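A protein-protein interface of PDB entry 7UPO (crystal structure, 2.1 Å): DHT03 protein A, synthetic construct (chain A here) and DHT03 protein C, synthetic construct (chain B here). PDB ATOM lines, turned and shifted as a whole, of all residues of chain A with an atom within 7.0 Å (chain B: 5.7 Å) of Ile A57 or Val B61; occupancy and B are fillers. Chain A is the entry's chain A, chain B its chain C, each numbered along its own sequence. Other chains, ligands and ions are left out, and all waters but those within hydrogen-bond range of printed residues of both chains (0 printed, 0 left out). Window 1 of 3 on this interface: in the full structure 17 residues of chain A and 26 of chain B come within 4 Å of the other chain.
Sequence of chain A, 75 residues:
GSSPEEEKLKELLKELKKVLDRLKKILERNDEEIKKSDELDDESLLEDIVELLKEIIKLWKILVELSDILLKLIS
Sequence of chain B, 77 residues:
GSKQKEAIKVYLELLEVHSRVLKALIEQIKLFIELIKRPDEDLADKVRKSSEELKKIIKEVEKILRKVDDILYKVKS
Leu A53 touches Leu B14 (CD2 to CD1, 3.7 Å).
Leu A53 touches Leu B65.
CG1 of Val B61 touches CG1 of Ile A57 (3.6 Å).
CD1 of Ile A57 touches CG of Glu B62, at 3.7 Å.
Ile A57 touches Leu B65 (CD1 to CD2, 3.9 Å).
Ile B58 touches Trp A60.
Ile B58 touches Lys A61.
Of the printed residues of chain B, Leu A53 touches Leu B14 (3.7 Å) and Leu B65 (3.9 Å).
Ile A57 touches three residues of chain B.
Printed residues of chain A within 4 Å of Leu B14: Leu A53.
Printed residues of chain A within 4 Å of Glu B62: Ile A57 (3.7 Å) and Lys A61 (3.3 Å).
Printed residues of chain A within 4 Å of Leu B65: Leu A53 (3.9 Å) and Ile A57 (3.9 Å).
The nearest residue of chain B that does not touch Ile A57 is Ile B58 (4.5 Å).
The nearest residue of chain A that does not touch Val B61 is Leu A53 (4.1 Å).
The nearest printed residue of chain A that does not touch Leu B65 is Lys A54 (4.1 Å).
Hydrophobic or aromatic side chains of chain B within 4 Å of the printed part of chain A: Leu B14, Ile B58, Val B61 and Leu B65.
Of the 11 printed residues of chain A, 4 touch a printed residue of chain B.
Along chain A the printed residues that touch a printed residue of chain B span positions 53 to 61.
The side-chain amino group (NZ) of Lys B59 is in salt-bridge range of the side-chain carboxylate (OE1) of Glu B62 (3.4 Å).
The side-chain amino group of Lys A61 is in salt-bridge range of the side-chain carboxylate of Glu B62 (3.3 Å).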
ATOM      1  N   LEU A  52      -8.159  -5.579  -9.426  1.00  0.00           N
ATOM      2  CA  LEU A  52      -8.309  -7.023  -9.591  1.00  0.00           C
ATOM      3  C   LEU A  52      -9.517  -7.349 -10.458  1.00  0.00           C
ATOM      4  O   LEU A  52      -9.436  -8.181 -11.370  1.00  0.00           O
ATOM      5  CB  LEU A  52      -8.436  -7.700  -8.226  1.00  0.00           C
ATOM      6  CG  LEU A  52      -8.681  -9.211  -8.266  1.00  0.00           C
ATOM      7  CD1 LEU A  52      -7.442  -9.940  -8.763  1.00  0.00           C
ATOM      8  CD2 LEU A  52      -9.105  -9.731  -6.901  1.00  0.00           C
ATOM      9  N   LEU A  53     -10.651  -6.697 -10.189  1.00  0.00           N
ATOM     10  CA  LEU A  53     -11.870  -6.977 -10.942  1.00  0.00           C
ATOM     11  C   LEU A  53     -11.702  -6.645 -12.419  1.00  0.00           C
ATOM     12  O   LEU A  53     -12.243  -7.346 -13.283  1.00  0.00           O
ATOM     13  CB  LEU A  53     -13.041  -6.192 -10.350  1.00  0.00           C
ATOM     14  CG  LEU A  53     -13.478  -6.604  -8.943  1.00  0.00           C
ATOM     15  CD1 LEU A  53     -14.616  -5.721  -8.453  1.00  0.00           C
ATOM     16  CD2 LEU A  53     -13.885  -8.069  -8.920  1.00  0.00           C
ATOM     17  N   LYS A  54     -10.954  -5.582 -12.729  1.00  0.00           N
ATOM     18  CA  LYS A  54     -10.765  -5.190 -14.124  1.00  0.00           C
ATOM     19  C   LYS A  54     -10.030  -6.271 -14.910  1.00  0.00           C
ATOM     20  O   LYS A  54     -10.447  -6.644 -16.013  1.00  0.00           O
ATOM     21  CB  LYS A  54     -10.012  -3.864 -14.199  1.00  0.00           C
ATOM     22  CG  LYS A  54     -10.839  -2.665 -13.762  1.00  0.00           C
ATOM     23  CD  LYS A  54     -10.045  -1.370 -13.852  1.00  0.00           C
ATOM     24  CE  LYS A  54     -10.938  -0.177 -13.577  1.00  0.00           C
ATOM     25  NZ  LYS A  54     -12.141  -0.188 -14.456  1.00  0.00           N
ATOM     26  N   GLU A  55      -8.924  -6.779 -14.362  1.00  0.00           N
ATOM     27  CA  GLU A  55      -8.198  -7.848 -15.042  1.00  0.00           C
ATOM     28  C   GLU A  55      -9.024  -9.126 -15.104  1.00  0.00           C
ATOM     29  O   GLU A  55      -9.004  -9.837 -16.115  1.00  0.00           O
ATOM     30  CB  GLU A  55      -6.863  -8.107 -14.346  1.00  0.00           C
ATOM     31  CG  GLU A  55      -5.814  -7.064 -14.657  1.00  0.00           C
ATOM     32  CD  GLU A  55      -5.368  -7.106 -16.101  1.00  0.00           C
ATOM     33  OE1 GLU A  55      -5.346  -8.209 -16.685  1.00  0.00           O
ATOM     34  OE2 GLU A  55      -5.041  -6.036 -16.656  1.00  0.00           O
ATOM     35  N   ILE A  56      -9.754  -9.432 -14.030  1.00  0.00           N
ATOM     36  CA  ILE A  56     -10.605 -10.618 -14.013  1.00  0.00           C
ATOM     37  C   ILE A  56     -11.657 -10.535 -15.112  1.00  0.00           C
ATOM     38  O   ILE A  56     -11.945 -11.527 -15.793  1.00  0.00           O
ATOM     39  CB  ILE A  56     -11.236 -10.787 -12.618  1.00  0.00           C
ATOM     40  CG1 ILE A  56     -10.278 -11.531 -11.690  1.00  0.00           C
ATOM     41  CG2 ILE A  56     -12.565 -11.507 -12.699  1.00  0.00           C
ATOM     42  CD1 ILE A  56      -9.965 -12.939 -12.147  1.00  0.00           C
ATOM     43  N   ILE A  57     -12.230  -9.347 -15.317  1.00  0.00           N
ATOM     44  CA  ILE A  57     -13.234  -9.172 -16.363  1.00  0.00           C
ATOM     45  C   ILE A  57     -12.612  -9.352 -17.742  1.00  0.00           C
ATOM     46  O   ILE A  57     -13.191 -10.010 -18.616  1.00  0.00           O
ATOM     47  CB  ILE A  57     -13.916  -7.800 -16.217  1.00  0.00           C
ATOM     48  CG1 ILE A  57     -14.849  -7.801 -15.006  1.00  0.00           C
ATOM     49  CG2 ILE A  57     -14.683  -7.445 -17.478  1.00  0.00           C
ATOM     50  CD1 ILE A  57     -15.424  -6.445 -14.674  1.00  0.00           C
ATOM     51  N   LYS A  58     -11.430  -8.772 -17.965  1.00  0.00           N
ATOM     52  CA  LYS A  58     -10.741  -8.972 -19.237  1.00  0.00           C
ATOM     53  C   LYS A  58     -10.402 -10.440 -19.450  1.00  0.00           C
ATOM     54  O   LYS A  58     -10.487 -10.949 -20.575  1.00  0.00           O
ATOM     55  CB  LYS A  58      -9.475  -8.116 -19.291  1.00  0.00           C
ATOM     56  CG  LYS A  58      -9.742  -6.645 -19.535  1.00  0.00           C
ATOM     57  CD  LYS A  58      -8.456  -5.840 -19.567  1.00  0.00           C
ATOM     58  CE  LYS A  58      -7.847  -5.714 -18.183  1.00  0.00           C
ATOM     59  NZ  LYS A  58      -6.660  -4.812 -18.183  1.00  0.00           N
ATOM     60  N   LEU A  59     -10.021 -11.137 -18.380  1.00  0.00           N
ATOM     61  CA  LEU A  59      -9.699 -12.556 -18.477  1.00  0.00           C
ATOM     62  C   LEU A  59     -10.880 -13.351 -19.022  1.00  0.00           C
ATOM     63  O   LEU A  59     -10.750 -14.078 -20.015  1.00  0.00           O
ATOM     64  CB  LEU A  59      -9.273 -13.076 -17.104  1.00  0.00           C
ATOM     65  CG  LEU A  59      -8.901 -14.553 -16.978  1.00  0.00           C
ATOM     66  CD1 LEU A  59      -7.749 -14.897 -17.906  1.00  0.00           C
ATOM     67  CD2 LEU A  59      -8.543 -14.874 -15.538  1.00  0.00           C
ATOM     68  N   TRP A  60     -12.050 -13.214 -18.388  1.00  0.00           N
ATOM     69  CA  TRP A  60     -13.218 -13.977 -18.826  1.00  0.00           C
ATOM     70  C   TRP A  60     -13.601 -13.633 -20.259  1.00  0.00           C
ATOM     71  O   TRP A  60     -14.014 -14.512 -21.026  1.00  0.00           O
ATOM     72  CB  TRP A  60     -14.412 -13.730 -17.903  1.00  0.00           C
ATOM     73  CG  TRP A  60     -14.196 -13.884 -16.416  1.00  0.00           C
ATOM     74  CD1 TRP A  60     -14.848 -13.192 -15.434  1.00  0.00           C
ATOM     75  CD2 TRP A  60     -13.304 -14.786 -15.739  1.00  0.00           C
ATOM     76  NE1 TRP A  60     -14.418 -13.600 -14.198  1.00  0.00           N
ATOM     77  CE2 TRP A  60     -13.468 -14.572 -14.354  1.00  0.00           C
ATOM     78  CE3 TRP A  60     -12.381 -15.747 -16.165  1.00  0.00           C
ATOM     79  CZ2 TRP A  60     -12.745 -15.279 -13.397  1.00  0.00           C
ATOM     80  CZ3 TRP A  60     -11.664 -16.448 -15.212  1.00  0.00           C
ATOM     81  CH2 TRP A  60     -11.850 -16.209 -13.844  1.00  0.00           C
ATOM     82  N   LYS A  61     -13.488 -12.356 -20.634  1.00  0.00           N
ATOM     83  CA  LYS A  61     -13.858 -11.948 -21.985  1.00  0.00           C
ATOM     84  C   LYS A  61     -12.995 -12.646 -23.029  1.00  0.00           C
ATOM     85  O   LYS A  61     -13.482 -13.003 -24.109  1.00  0.00           O
ATOM     86  CB  LYS A  61     -13.751 -10.428 -22.123  1.00  0.00           C
ATOM     87  CG  LYS A  61     -14.849  -9.650 -21.408  1.00  0.00           C
ATOM     88  CD  LYS A  61     -14.656  -8.147 -21.588  1.00  0.00           C
ATOM     89  CE  LYS A  61     -15.766  -7.346 -20.920  1.00  0.00           C
ATOM     90  NZ  LYS A  61     -17.070  -7.452 -21.633  1.00  0.00           N
ATOM     91  N   ILE A  62     -11.714 -12.858 -22.724  1.00  0.00           N
ATOM     92  CA  ILE A  62     -10.841 -13.557 -23.661  1.00  0.00           C
ATOM     93  C   ILE A  62     -11.197 -15.037 -23.715  1.00  0.00           C
ATOM     94  O   ILE A  62     -11.149 -15.662 -24.782  1.00  0.00           O
ATOM     95  CB  ILE A  62      -9.364 -13.339 -23.286  1.00  0.00           C
ATOM     96  CG1 ILE A  62      -9.024 -11.848 -23.319  1.00  0.00           C
ATOM     97  CG2 ILE A  62      -8.450 -14.100 -24.233  1.00  0.00           C
ATOM     98  CD1 ILE A  62      -7.605 -11.536 -22.903  1.00  0.00           C
ATOM     99  N   LEU B  14     -17.558 -12.479  -4.601  1.00  0.00           N
ATOM    100  CA  LEU B  14     -16.619 -13.029  -5.573  1.00  0.00           C
ATOM    101  C   LEU B  14     -16.440 -14.532  -5.390  1.00  0.00           C
ATOM    102  O   LEU B  14     -16.295 -15.266  -6.374  1.00  0.00           O
ATOM    103  CB  LEU B  14     -15.272 -12.315  -5.470  1.00  0.00           C
ATOM    104  CG  LEU B  14     -15.005 -11.235  -6.517  1.00  0.00           C
ATOM    105  CD1 LEU B  14     -13.588 -10.706  -6.387  1.00  0.00           C
ATOM    106  CD2 LEU B  14     -15.243 -11.788  -7.909  1.00  0.00           C
ATOM    107  N   VAL B  17     -19.256 -16.180  -7.023  1.00  0.00           N
ATOM    108  CA  VAL B  17     -19.121 -16.024  -8.468  1.00  0.00           C
ATOM    109  C   VAL B  17     -18.036 -16.951  -9.003  1.00  0.00           C
ATOM    110  O   VAL B  17     -18.245 -17.681  -9.978  1.00  0.00           O
ATOM    111  CB  VAL B  17     -18.830 -14.553  -8.821  1.00  0.00           C
ATOM    112  CG1 VAL B  17     -18.326 -14.435 -10.244  1.00  0.00           C
ATOM    113  CG2 VAL B  17     -20.076 -13.708  -8.632  1.00  0.00           C
ATOM    114  N   LYS B  56     -22.972 -14.329 -18.738  1.00  0.00           N
ATOM    115  CA  LYS B  56     -23.785 -13.784 -17.657  1.00  0.00           C
ATOM    116  C   LYS B  56     -22.960 -13.560 -16.398  1.00  0.00           C
ATOM    117  O   LYS B  56     -23.218 -12.611 -15.649  1.00  0.00           O
ATOM    118  CB  LYS B  56     -24.960 -14.709 -17.350  1.00  0.00           C
ATOM    119  CG  LYS B  56     -25.875 -14.988 -18.529  1.00  0.00           C
ATOM    120  CD  LYS B  56     -27.152 -15.677 -18.070  1.00  0.00           C
ATOM    121  CE  LYS B  56     -26.841 -16.856 -17.157  1.00  0.00           C
ATOM    122  NZ  LYS B  56     -28.067 -17.415 -16.524  1.00  0.00           N
ATOM    123  N   ILE B  57     -21.971 -14.421 -16.146  1.00  0.00           N
ATOM    124  CA  ILE B  57     -21.094 -14.222 -14.999  1.00  0.00           C
ATOM    125  C   ILE B  57     -20.263 -12.960 -15.179  1.00  0.00           C
ATOM    126  O   ILE B  57     -20.037 -12.208 -14.222  1.00  0.00           O
ATOM    127  CB  ILE B  57     -20.208 -15.461 -14.779  1.00  0.00           C
ATOM    128  CG1 ILE B  57     -21.066 -16.643 -14.327  1.00  0.00           C
ATOM    129  CG2 ILE B  57     -19.122 -15.162 -13.763  1.00  0.00           C
ATOM    130  CD1 ILE B  57     -20.290 -17.923 -14.112  1.00  0.00           C
ATOM    131  N   ILE B  58     -19.798 -12.706 -16.405  1.00  0.00           N
ATOM    132  CA  ILE B  58     -19.093 -11.458 -16.699  1.00  0.00           C
ATOM    133  C   ILE B  58     -19.954 -10.266 -16.309  1.00  0.00           C
ATOM    134  O   ILE B  58     -19.484  -9.320 -15.661  1.00  0.00           O
ATOM    135  CB  ILE B  58     -18.696 -11.404 -18.185  1.00  0.00           C
ATOM    136  CG1 ILE B  58     -17.629 -12.455 -18.488  1.00  0.00           C
ATOM    137  CG2 ILE B  58     -18.210 -10.008 -18.560  1.00  0.00           C
ATOM    138  CD1 ILE B  58     -17.240 -12.543 -19.949  1.00  0.00           C
ATOM    139  N   LYS B  59     -21.236 -10.298 -16.684  1.00  0.00           N
ATOM    140  CA  LYS B  59     -22.129  -9.193 -16.354  1.00  0.00           C
ATOM    141  C   LYS B  59     -22.291  -9.044 -14.846  1.00  0.00           C
ATOM    142  O   LYS B  59     -22.418  -7.925 -14.336  1.00  0.00           O
ATOM    143  CB  LYS B  59     -23.483  -9.396 -17.033  1.00  0.00           C
ATOM    144  CG  LYS B  59     -23.406  -9.422 -18.552  1.00  0.00           C
ATOM    145  CD  LYS B  59     -22.768  -8.148 -19.078  1.00  0.00           C
ATOM    146  CE  LYS B  59     -22.535  -8.203 -20.578  1.00  0.00           C
ATOM    147  NZ  LYS B  59     -21.883  -6.956 -21.065  1.00  0.00           N
ATOM    148  N   GLU B  60     -22.278 -10.162 -14.115  1.00  0.00           N
ATOM    149  CA  GLU B  60     -22.359 -10.085 -12.660  1.00  0.00           C
ATOM    150  C   GLU B  60     -21.106  -9.454 -12.074  1.00  0.00           C
ATOM    151  O   GLU B  60     -21.180  -8.711 -11.091  1.00  0.00           O
ATOM    152  CB  GLU B  60     -22.576 -11.476 -12.068  1.00  0.00           C
ATOM    153  CG  GLU B  60     -23.862 -12.147 -12.498  1.00  0.00           C
ATOM    154  CD  GLU B  60     -24.059 -13.486 -11.824  1.00  0.00           C
ATOM    155  OE1 GLU B  60     -23.296 -13.789 -10.884  1.00  0.00           O
ATOM    156  OE2 GLU B  60     -24.971 -14.234 -12.231  1.00  0.00           O
ATOM    157  N   VAL B  61     -19.941  -9.746 -12.656  1.00  0.00           N
ATOM    158  CA  VAL B  61     -18.707  -9.159 -12.149  1.00  0.00           C
ATOM    159  C   VAL B  61     -18.629  -7.682 -12.517  1.00  0.00           C
ATOM    160  O   VAL B  61     -18.080  -6.874 -11.758  1.00  0.00           O
ATOM    161  CB  VAL B  61     -17.489  -9.948 -12.669  1.00  0.00           C
ATOM    162  CG1 VAL B  61     -16.199  -9.372 -12.103  1.00  0.00           C
ATOM    163  CG2 VAL B  61     -17.614 -11.420 -12.297  1.00  0.00           C
ATOM    164  N   GLU B  62     -19.183  -7.299 -13.670  1.00  0.00           N
ATOM    165  CA  GLU B  62     -19.237  -5.886 -14.026  1.00  0.00           C
ATOM    166  C   GLU B  62     -20.166  -5.123 -13.092  1.00  0.00           C
ATOM    167  O   GLU B  62     -19.910  -3.956 -12.773  1.00  0.00           O
ATOM    168  CB  GLU B  62     -19.681  -5.726 -15.479  1.00  0.00           C
ATOM    169  CG  GLU B  62     -18.673  -6.239 -16.497  1.00  0.00           C
ATOM    170  CD  GLU B  62     -19.203  -6.202 -17.915  1.00  0.00           C
ATOM    171  OE1 GLU B  62     -20.438  -6.178 -18.088  1.00  0.00           O
ATOM    172  OE2 GLU B  62     -18.383  -6.191 -18.858  1.00  0.00           O
ATOM    173  N   LYS B  63     -21.251  -5.765 -12.645  1.00  0.00           N
ATOM    174  CA  LYS B  63     -22.130  -5.129 -11.669  1.00  0.00           C
ATOM    175  C   LYS B  63     -21.428  -4.958 -10.329  1.00  0.00           C
ATOM    176  O   LYS B  63     -21.549  -3.908  -9.688  1.00  0.00           O
ATOM    177  CB  LYS B  63     -23.418  -5.937 -11.505  1.00  0.00           C
ATOM    178  CG  LYS B  63     -24.323  -5.425 -10.386  1.00  0.00           C
ATOM    179  CD  LYS B  63     -25.793  -5.763 -10.618  1.00  0.00           C
ATOM    180  CE  LYS B  63     -26.073  -7.248 -10.464  1.00  0.00           C
ATOM    181  NZ  LYS B  63     -27.531  -7.545 -10.573  1.00  0.00           N
ATOM    182  N   ILE B  64     -20.686  -5.978  -9.890  1.00  0.00           N
ATOM    183  CA  ILE B  64     -19.889  -5.852  -8.672  1.00  0.00           C
ATOM    184  C   ILE B  64     -18.916  -4.688  -8.795  1.00  0.00           C
ATOM    185  O   ILE B  64     -18.765  -3.883  -7.870  1.00  0.00           O
ATOM    186  CB  ILE B  64     -19.157  -7.175  -8.370  1.00  0.00           C
ATOM    187  CG1 ILE B  64     -20.156  -8.293  -8.073  1.00  0.00           C
ATOM    188  CG2 ILE B  64     -18.197  -7.003  -7.199  1.00  0.00           C
ATOM    189  CD1 ILE B  64     -19.506  -9.626  -7.757  1.00  0.00           C
ATOM    190  N   LEU B  65     -18.254  -4.568  -9.949  1.00  0.00           N
ATOM    191  CA  LEU B  65     -17.280  -3.501 -10.140  1.00  0.00           C
ATOM    192  C   LEU B  65     -17.948  -2.131 -10.093  1.00  0.00           C
ATOM    193  O   LEU B  65     -17.434  -1.204  -9.458  1.00  0.00           O
ATOM    194  CB  LEU B  65     -16.535  -3.699 -11.461  1.00  0.00           C
ATOM    195  CG  LEU B  65     -15.558  -2.583 -11.838  1.00  0.00           C
ATOM    196  CD1 LEU B  65     -14.557  -2.346 -10.720  1.00  0.00           C
ATOM    197  CD2 LEU B  65     -14.841  -2.911 -13.140  1.00  0.00           C
ATOM    198  N   ARG B  66     -19.096  -1.985 -10.764  1.00  0.00           N
ATOM    199  CA  ARG B  66     -19.809  -0.710 -10.736  1.00  0.00           C
ATOM    200  C   ARG B  66     -20.176  -0.314  -9.315  1.00  0.00           C
ATOM    201  O   ARG B  66     -20.027   0.852  -8.928  1.00  0.00           O
ATOM    202  CB  ARG B  66     -21.067  -0.782 -11.601  1.00  0.00           C
ATOM    203  CG  ARG B  66     -20.822  -0.605 -13.086  1.00  0.00           C
ATOM    204  CD  ARG B  66     -22.128  -0.373 -13.831  1.00  0.00           C
ATOM    205  NE  ARG B  66     -23.087  -1.447 -13.601  1.00  0.00           N
ATOM    206  CZ  ARG B  66     -23.111  -2.584 -14.286  1.00  0.00           C
ATOM    207  NH1 ARG B  66     -22.222  -2.800 -15.249  1.00  0.00           N
ATOM    208  NH2 ARG B  66     -24.022  -3.509 -14.010  1.00  0.00           N
